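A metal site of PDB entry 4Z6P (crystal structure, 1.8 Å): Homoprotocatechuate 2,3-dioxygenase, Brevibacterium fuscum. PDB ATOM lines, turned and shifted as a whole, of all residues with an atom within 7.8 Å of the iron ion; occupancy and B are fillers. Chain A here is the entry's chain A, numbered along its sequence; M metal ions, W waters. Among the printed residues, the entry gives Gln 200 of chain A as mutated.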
ATOM      1  N   ASP A 154      36.457   8.018 -24.462  1.00  0.00           N
ATOM      2  CA  ASP A 154      36.337   6.847 -23.616  1.00  0.00           C
ATOM      3  C   ASP A 154      36.637   5.514 -24.309  1.00  0.00           C
ATOM      4  O   ASP A 154      37.393   4.708 -23.755  1.00  0.00           O
ATOM      5  CB  ASP A 154      34.983   6.719 -22.909  1.00  0.00           C
ATOM      6  CG  ASP A 154      35.028   5.658 -21.788  1.00  0.00           C
ATOM      7  OD1 ASP A 154      35.645   5.941 -20.740  1.00  0.00           O
ATOM      8  OD2 ASP A 154      34.513   4.513 -21.977  1.00  0.00           O
ATOM      9  N   HIS A 155      35.984   5.234 -25.427  1.00  0.00           N
ATOM     10  CA  HIS A 155      36.130   3.917 -26.078  1.00  0.00           C
ATOM     11  C   HIS A 155      35.669   3.920 -27.503  1.00  0.00           C
ATOM     12  O   HIS A 155      35.026   4.863 -27.964  1.00  0.00           O
ATOM     13  CB  HIS A 155      35.367   2.831 -25.293  1.00  0.00           C
ATOM     14  CG  HIS A 155      33.870   2.986 -25.270  1.00  0.00           C
ATOM     15  ND1 HIS A 155      33.216   3.619 -24.240  1.00  0.00           N
ATOM     16  CD2 HIS A 155      32.900   2.531 -26.103  1.00  0.00           C
ATOM     17  CE1 HIS A 155      31.901   3.533 -24.440  1.00  0.00           C
ATOM     18  NE2 HIS A 155      31.685   2.888 -25.558  1.00  0.00           N
ATOM     19  N   PHE A 156      36.002   2.831 -28.202  1.00  0.00           N
ATOM     20  CA  PHE A 156      35.474   2.461 -29.483  1.00  0.00           C
ATOM     21  C   PHE A 156      34.566   1.231 -29.321  1.00  0.00           C
ATOM     22  O   PHE A 156      34.670   0.500 -28.313  1.00  0.00           O
ATOM     23  CB  PHE A 156      36.607   2.057 -30.408  1.00  0.00           C
ATOM     24  CG  PHE A 156      37.760   3.022 -30.479  1.00  0.00           C
ATOM     25  CD1 PHE A 156      37.566   4.370 -30.821  1.00  0.00           C
ATOM     26  CD2 PHE A 156      39.058   2.573 -30.279  1.00  0.00           C
ATOM     27  CE1 PHE A 156      38.659   5.238 -30.937  1.00  0.00           C
ATOM     28  CE2 PHE A 156      40.141   3.434 -30.369  1.00  0.00           C
ATOM     29  CZ  PHE A 156      39.937   4.771 -30.695  1.00  0.00           C
ATOM     30  N   ASN A 157      33.690   0.989 -30.276  1.00  0.00           N
ATOM     31  CA  ASN A 157      32.911  -0.258 -30.279  1.00  0.00           C
ATOM     32  C   ASN A 157      32.825  -0.757 -31.729  1.00  0.00           C
ATOM     33  O   ASN A 157      32.429  -0.019 -32.628  1.00  0.00           O
ATOM     34  CB  ASN A 157      31.536  -0.024 -29.669  1.00  0.00           C
ATOM     35  CG  ASN A 157      30.717  -1.295 -29.529  1.00  0.00           C
ATOM     36  OD1 ASN A 157      30.488  -1.985 -30.515  1.00  0.00           O
ATOM     37  ND2 ASN A 157      30.255  -1.577 -28.321  1.00  0.00           N
ATOM     38  N   TRP A 192      33.089  -6.585 -23.733  1.00  0.00           N
ATOM     39  CA  TRP A 192      33.674  -5.286 -23.472  1.00  0.00           C
ATOM     40  C   TRP A 192      35.053  -5.569 -22.883  1.00  0.00           C
ATOM     41  O   TRP A 192      35.196  -6.453 -22.044  1.00  0.00           O
ATOM     42  CB  TRP A 192      32.798  -4.563 -22.438  1.00  0.00           C
ATOM     43  CG  TRP A 192      31.513  -4.001 -22.981  1.00  0.00           C
ATOM     44  CD1 TRP A 192      31.258  -2.697 -23.226  1.00  0.00           C
ATOM     45  CD2 TRP A 192      30.292  -4.704 -23.315  1.00  0.00           C
ATOM     46  NE1 TRP A 192      29.990  -2.527 -23.713  1.00  0.00           N
ATOM     47  CE2 TRP A 192      29.377  -3.738 -23.795  1.00  0.00           C
ATOM     48  CE3 TRP A 192      29.905  -6.031 -23.256  1.00  0.00           C
ATOM     49  CZ2 TRP A 192      28.086  -4.047 -24.198  1.00  0.00           C
ATOM     50  CZ3 TRP A 192      28.640  -6.366 -23.679  1.00  0.00           C
ATOM     51  CH2 TRP A 192      27.726  -5.363 -24.133  1.00  0.00           C
ATOM     52  N   GLN A 200      36.047  -0.247 -20.566  1.00  0.00           N
ATOM     53  CA  GLN A 200      36.340  -0.514 -21.960  1.00  0.00           C
ATOM     54  C   GLN A 200      37.280   0.520 -22.560  1.00  0.00           C
ATOM     55  O   GLN A 200      37.206   1.701 -22.218  1.00  0.00           O
ATOM     56  CB  GLN A 200      35.061  -0.597 -22.793  1.00  0.00           C
ATOM     57  CG  GLN A 200      34.100   0.576 -22.553  1.00  0.00           C
ATOM     58  CD  GLN A 200      32.717   0.442 -23.143  1.00  0.00           C
ATOM     59  OE1 GLN A 200      31.714   0.886 -22.533  1.00  0.00           O
ATOM     60  NE2 GLN A 200      32.645  -0.067 -24.321  1.00  0.00           N
ATOM     61  N   ALA A 203      35.294  -2.583 -27.647  1.00  0.00           N
ATOM     62  CA  ALA A 203      34.225  -3.500 -27.329  1.00  0.00           C
ATOM     63  C   ALA A 203      33.773  -4.119 -28.633  1.00  0.00           C
ATOM     64  O   ALA A 203      33.927  -3.522 -29.691  1.00  0.00           O
ATOM     65  CB  ALA A 203      33.068  -2.778 -26.658  1.00  0.00           C
ATOM     66  N   THR A 205      30.626  -5.935 -30.724  1.00  0.00           N
ATOM     67  CA  THR A 205      29.204  -6.164 -30.881  1.00  0.00           C
ATOM     68  C   THR A 205      29.056  -7.163 -32.015  1.00  0.00           C
ATOM     69  O   THR A 205      29.616  -6.959 -33.094  1.00  0.00           O
ATOM     70  CB  THR A 205      28.477  -4.864 -31.261  1.00  0.00           C
ATOM     71  OG1 THR A 205      28.641  -3.901 -30.209  1.00  0.00           O
ATOM     72  CG2 THR A 205      26.983  -5.137 -31.532  1.00  0.00           C
ATOM     73  N   HIS A 213      30.845   0.474 -34.778  1.00  0.00           N
ATOM     74  CA  HIS A 213      29.545   0.741 -34.215  1.00  0.00           C
ATOM     75  C   HIS A 213      29.431   2.177 -33.676  1.00  0.00           C
ATOM     76  O   HIS A 213      28.498   2.913 -34.047  1.00  0.00           O
ATOM     77  CB  HIS A 213      29.227  -0.257 -33.125  1.00  0.00           C
ATOM     78  CG  HIS A 213      27.785  -0.260 -32.792  1.00  0.00           C
ATOM     79  ND1 HIS A 213      27.225   0.679 -31.962  1.00  0.00           N
ATOM     80  CD2 HIS A 213      26.766  -1.023 -33.257  1.00  0.00           C
ATOM     81  CE1 HIS A 213      25.922   0.468 -31.891  1.00  0.00           C
ATOM     82  NE2 HIS A 213      25.625  -0.561 -32.660  1.00  0.00           N
ATOM     83  N   HIS A 214      30.391   2.559 -32.853  1.00  0.00           N
ATOM     84  CA  HIS A 214      30.482   3.929 -32.342  1.00  0.00           C
ATOM     85  C   HIS A 214      31.848   4.292 -31.774  1.00  0.00           C
ATOM     86  O   HIS A 214      32.667   3.446 -31.442  1.00  0.00           O
ATOM     87  CB  HIS A 214      29.391   4.216 -31.282  1.00  0.00           C
ATOM     88  CG  HIS A 214      29.403   3.305 -30.102  1.00  0.00           C
ATOM     89  ND1 HIS A 214      28.638   2.165 -30.045  1.00  0.00           N
ATOM     90  CD2 HIS A 214      30.027   3.387 -28.901  1.00  0.00           C
ATOM     91  CE1 HIS A 214      28.798   1.558 -28.883  1.00  0.00           C
ATOM     92  NE2 HIS A 214      29.637   2.285 -28.163  1.00  0.00           N
ATOM     93  N   VAL A 215      31.994   5.607 -31.612  1.00  0.00           N
ATOM     94  CA  VAL A 215      33.011   6.199 -30.777  1.00  0.00           C
ATOM     95  C   VAL A 215      32.323   6.874 -29.591  1.00  0.00           C
ATOM     96  O   VAL A 215      31.295   7.512 -29.752  1.00  0.00           O
ATOM     97  CB  VAL A 215      33.788   7.284 -31.572  1.00  0.00           C
ATOM     98  CG1 VAL A 215      34.854   7.924 -30.703  1.00  0.00           C
ATOM     99  CG2 VAL A 215      34.403   6.688 -32.853  1.00  0.00           C
ATOM    100  N   ALA A 216      32.884   6.713 -28.398  1.00  0.00           N
ATOM    101  CA  ALA A 216      32.275   7.238 -27.182  1.00  0.00           C
ATOM    102  C   ALA A 216      33.129   8.287 -26.515  1.00  0.00           C
ATOM    103  O   ALA A 216      34.338   8.079 -26.300  1.00  0.00           O
ATOM    104  CB  ALA A 216      31.988   6.109 -26.195  1.00  0.00           C
ATOM    105  N   HIS A 248      22.961   2.151 -18.689  1.00  0.00           N
ATOM    106  CA  HIS A 248      23.340   0.824 -19.150  1.00  0.00           C
ATOM    107  C   HIS A 248      23.288  -0.196 -18.019  1.00  0.00           C
ATOM    108  O   HIS A 248      23.556   0.149 -16.845  1.00  0.00           O
ATOM    109  CB  HIS A 248      24.782   0.818 -19.668  1.00  0.00           C
ATOM    110  CG  HIS A 248      24.995   1.384 -21.042  1.00  0.00           C
ATOM    111  ND1 HIS A 248      24.264   0.982 -22.148  1.00  0.00           N
ATOM    112  CD2 HIS A 248      25.913   2.272 -21.494  1.00  0.00           C
ATOM    113  CE1 HIS A 248      24.706   1.620 -23.217  1.00  0.00           C
ATOM    114  NE2 HIS A 248      25.704   2.402 -22.850  1.00  0.00           N
ATOM    115  N   VAL A 250      25.124  -3.405 -18.641  1.00  0.00           N
ATOM    116  CA  VAL A 250      26.515  -3.607 -18.911  1.00  0.00           C
ATOM    117  C   VAL A 250      27.224  -2.236 -18.847  1.00  0.00           C
ATOM    118  O   VAL A 250      26.877  -1.321 -19.597  1.00  0.00           O
ATOM    119  CB  VAL A 250      26.749  -4.142 -20.334  1.00  0.00           C
ATOM    120  CG1 VAL A 250      28.247  -4.149 -20.638  1.00  0.00           C
ATOM    121  CG2 VAL A 250      26.167  -5.557 -20.483  1.00  0.00           C
ATOM    122  N   SER A 251      28.243  -2.134 -17.999  1.00  0.00           N
ATOM    123  CA  SER A 251      29.065  -0.891 -17.781  1.00  0.00           C
ATOM    124  C   SER A 251      28.525   0.009 -16.676  1.00  0.00           C
ATOM    125  O   SER A 251      29.290   0.792 -16.129  1.00  0.00           O
ATOM    126  CB  SER A 251      29.350  -0.047 -19.032  1.00  0.00           C
ATOM    127  OG  SER A 251      28.264   0.835 -19.378  1.00  0.00           O
ATOM    128  N   TYR A 255      24.223   7.034 -20.437  1.00  0.00           N
ATOM    129  CA  TYR A 255      24.560   7.034 -21.879  1.00  0.00           C
ATOM    130  C   TYR A 255      23.534   7.715 -22.771  1.00  0.00           C
ATOM    131  O   TYR A 255      22.353   7.920 -22.374  1.00  0.00           O
ATOM    132  CB  TYR A 255      24.757   5.574 -22.383  1.00  0.00           C
ATOM    133  CG  TYR A 255      23.447   4.842 -22.572  1.00  0.00           C
ATOM    134  CD1 TYR A 255      22.719   4.969 -23.765  1.00  0.00           C
ATOM    135  CD2 TYR A 255      22.930   4.042 -21.572  1.00  0.00           C
ATOM    136  CE1 TYR A 255      21.496   4.303 -23.939  1.00  0.00           C
ATOM    137  CE2 TYR A 255      21.698   3.389 -21.730  1.00  0.00           C
ATOM    138  CZ  TYR A 255      20.996   3.503 -22.917  1.00  0.00           C
ATOM    139  OH  TYR A 255      19.798   2.837 -23.056  1.00  0.00           O
ATOM    140  N   LEU A 256      23.971   7.998 -24.013  1.00  0.00           N
ATOM    141  CA  LEU A 256      23.188   8.575 -25.102  1.00  0.00           C
ATOM    142  C   LEU A 256      23.866   8.184 -26.403  1.00  0.00           C
ATOM    143  O   LEU A 256      25.097   8.271 -26.483  1.00  0.00           O
ATOM    144  CB  LEU A 256      23.185  10.110 -24.996  1.00  0.00           C
ATOM    145  CG  LEU A 256      22.505  10.883 -26.098  1.00  0.00           C
ATOM    146  CD1 LEU A 256      21.007  10.598 -26.042  1.00  0.00           C
ATOM    147  CD2 LEU A 256      22.812  12.361 -25.965  1.00  0.00           C
ATOM    148  N   TYR A 257      23.094   7.850 -27.443  1.00  0.00           N
ATOM    149  CA  TYR A 257      23.645   7.623 -28.781  1.00  0.00           C
ATOM    150  C   TYR A 257      23.012   8.630 -29.750  1.00  0.00           C
ATOM    151  O   TYR A 257      21.776   8.726 -29.857  1.00  0.00           O
ATOM    152  CB  TYR A 257      23.351   6.216 -29.292  1.00  0.00           C
ATOM    153  CG  TYR A 257      23.938   5.146 -28.439  1.00  0.00           C
ATOM    154  CD1 TYR A 257      25.235   4.746 -28.605  1.00  0.00           C
ATOM    155  CD2 TYR A 257      23.183   4.527 -27.455  1.00  0.00           C
ATOM    156  CE1 TYR A 257      25.791   3.755 -27.790  1.00  0.00           C
ATOM    157  CE2 TYR A 257      23.727   3.552 -26.649  1.00  0.00           C
ATOM    158  CZ  TYR A 257      25.030   3.180 -26.829  1.00  0.00           C
ATOM    159  OH  TYR A 257      25.539   2.190 -26.049  1.00  0.00           O
ATOM    160  N   GLU A 267      28.513   7.870 -28.957  1.00  0.00           N
ATOM    161  CA  GLU A 267      27.964   7.680 -27.641  1.00  0.00           C
ATOM    162  C   GLU A 267      28.516   8.767 -26.725  1.00  0.00           C
ATOM    163  O   GLU A 267      29.726   9.069 -26.753  1.00  0.00           O
ATOM    164  CB  GLU A 267      28.325   6.293 -27.097  1.00  0.00           C
ATOM    165  CG  GLU A 267      27.641   5.973 -25.778  1.00  0.00           C
ATOM    166  CD  GLU A 267      27.994   4.591 -25.237  1.00  0.00           C
ATOM    167  OE1 GLU A 267      28.870   3.956 -25.859  1.00  0.00           O
ATOM    168  OE2 GLU A 267      27.413   4.142 -24.197  1.00  0.00           O
ATOM    169  N   ILE A 268      27.645   9.270 -25.861  1.00  0.00           N
ATOM    170  CA  ILE A 268      28.040  10.054 -24.716  1.00  0.00           C
ATOM    171  C   ILE A 268      27.808   9.208 -23.452  1.00  0.00           C
ATOM    172  O   ILE A 268      26.812   8.504 -23.345  1.00  0.00           O
ATOM    173  CB  ILE A 268      27.269  11.395 -24.651  1.00  0.00           C
ATOM    174  CG1 ILE A 268      26.996  12.022 -26.037  1.00  0.00           C
ATOM    175  CG2 ILE A 268      28.019  12.404 -23.802  1.00  0.00           C
ATOM    176  CD1 ILE A 268      28.216  12.348 -26.854  1.00  0.00           C
ATOM    177  N   TYR A 269      28.771   9.208 -22.545  1.00  0.00           N
ATOM    178  CA  TYR A 269      28.908   8.144 -21.554  1.00  0.00           C
ATOM    179  C   TYR A 269      29.450   8.771 -20.273  1.00  0.00           C
ATOM    180  O   TYR A 269      30.360   9.603 -20.333  1.00  0.00           O
ATOM    181  CB  TYR A 269      29.902   7.174 -22.133  1.00  0.00           C
ATOM    182  CG  TYR A 269      30.332   5.928 -21.411  1.00  0.00           C
ATOM    183  CD1 TYR A 269      29.697   4.713 -21.669  1.00  0.00           C
ATOM    184  CD2 TYR A 269      31.442   5.928 -20.577  1.00  0.00           C
ATOM    185  CE1 TYR A 269      30.128   3.553 -21.089  1.00  0.00           C
ATOM    186  CE2 TYR A 269      31.885   4.760 -19.970  1.00  0.00           C
ATOM    187  CZ  TYR A 269      31.226   3.570 -20.263  1.00  0.00           C
ATOM    188  OH  TYR A 269      31.649   2.364 -19.738  1.00  0.00           O
ATOM    189  N   ARG A 293      21.045  -3.921 -21.418  1.00  0.00           N
ATOM    190  CA  ARG A 293      21.519  -2.837 -22.245  1.00  0.00           C
ATOM    191  C   ARG A 293      20.980  -1.479 -21.770  1.00  0.00           C
ATOM    192  O   ARG A 293      21.732  -0.542 -21.652  1.00  0.00           O
ATOM    193  CB  ARG A 293      21.162  -3.088 -23.722  1.00  0.00           C
ATOM    194  CG  ARG A 293      22.093  -4.090 -24.377  1.00  0.00           C
ATOM    195  CD  ARG A 293      22.059  -4.041 -25.889  1.00  0.00           C
ATOM    196  NE  ARG A 293      22.977  -5.024 -26.465  1.00  0.00           N
ATOM    197  CZ  ARG A 293      24.290  -4.852 -26.606  1.00  0.00           C
ATOM    198  NH1 ARG A 293      24.877  -3.733 -26.181  1.00  0.00           N
ATOM    199  NH2 ARG A 293      25.027  -5.792 -27.197  1.00  0.00           N
ATOM    200  N   TRP A 304      19.920   0.428 -33.925  1.00  0.00           N
ATOM    201  CA  TRP A 304      21.126   0.282 -33.084  1.00  0.00           C
ATOM    202  C   TRP A 304      21.841  -1.029 -33.354  1.00  0.00           C
ATOM    203  O   TRP A 304      23.086  -1.135 -33.253  1.00  0.00           O
ATOM    204  CB  TRP A 304      20.760   0.415 -31.584  1.00  0.00           C
ATOM    205  CG  TRP A 304      21.920   0.717 -30.716  1.00  0.00           C
ATOM    206  CD1 TRP A 304      22.388   1.944 -30.413  1.00  0.00           C
ATOM    207  CD2 TRP A 304      22.783  -0.222 -30.083  1.00  0.00           C
ATOM    208  NE1 TRP A 304      23.505   1.845 -29.620  1.00  0.00           N
ATOM    209  CE2 TRP A 304      23.764   0.515 -29.396  1.00  0.00           C
ATOM    210  CE3 TRP A 304      22.824  -1.620 -30.032  1.00  0.00           C
ATOM    211  CZ2 TRP A 304      24.778  -0.092 -28.662  1.00  0.00           C
ATOM    212  CZ3 TRP A 304      23.827  -2.220 -29.325  1.00  0.00           C
ATOM    213  CH2 TRP A 304      24.791  -1.453 -28.653  1.00  0.00           C
HETATM  214 FE    FE M   1      29.662   2.013 -25.934  1.00  0.00          FE
HETATM  215  O   HOH W   1      30.624  -0.005 -25.968  1.00  0.00           O
HETATM  216  O   HOH W   2      27.699   0.970 -26.206  1.00  0.00           O
HETATM  217  O   HOH W   3      29.260   1.800 -23.803  1.00  0.00           O
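Water W3 bridges the side-chain amide oxygen of Gln 200 (2.9 Å) and the side-chain carboxylate of Glu 267 (3.0 Å).
Residues that only touch the iron ion: Gln 200 (3.98 Å). Along chain A the residues within 4 Å of the iron ion span positions 155 to 267. The nearest printed residue that does not touch the iron ion is Tyr 257 (4.1 Å).
The iron ion is bound by OE1 of Glu 267 (2.1 Å), water W3 (2.2 Å), water W1 (2.2 Å), NE2 of His 155 (2.2 Å), water W2 (2.2 Å) and NE2 of His 214 (2.2 Å).
The side-chain carboxylate of Glu 267 is in hydrogen-bond range of the side-chain hydroxyl of Tyr 257 (3.3 Å). The side-chain carboxylate (OE2) of Glu 267 is in hydrogen-bond range of a ring nitrogen (NE2) of His 248 (2.8 Å). N of Glu 267 lies within hydrogen-bond range of O of Val 215. A ring nitrogen (NE2) of His 155 lies close to the side-chain amide nitrogen of Gln 200 (3.3 Å). O of His 155 sits at hydrogen-bond distance from N of Ala 216, 2.9 Å away. The side-chain carboxylate of Asp 154 lies within hydrogen-bond range of a ring nitrogen (ND1) of His 155 (2.8 Å). O of His 214 sits at hydrogen-bond distance from N of Asn 157 (2.9 Å). A ring nitrogen (ND1) of His 214 is in hydrogen-bond range of a ring nitrogen (ND1) of His 213, 2.8 Å away.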
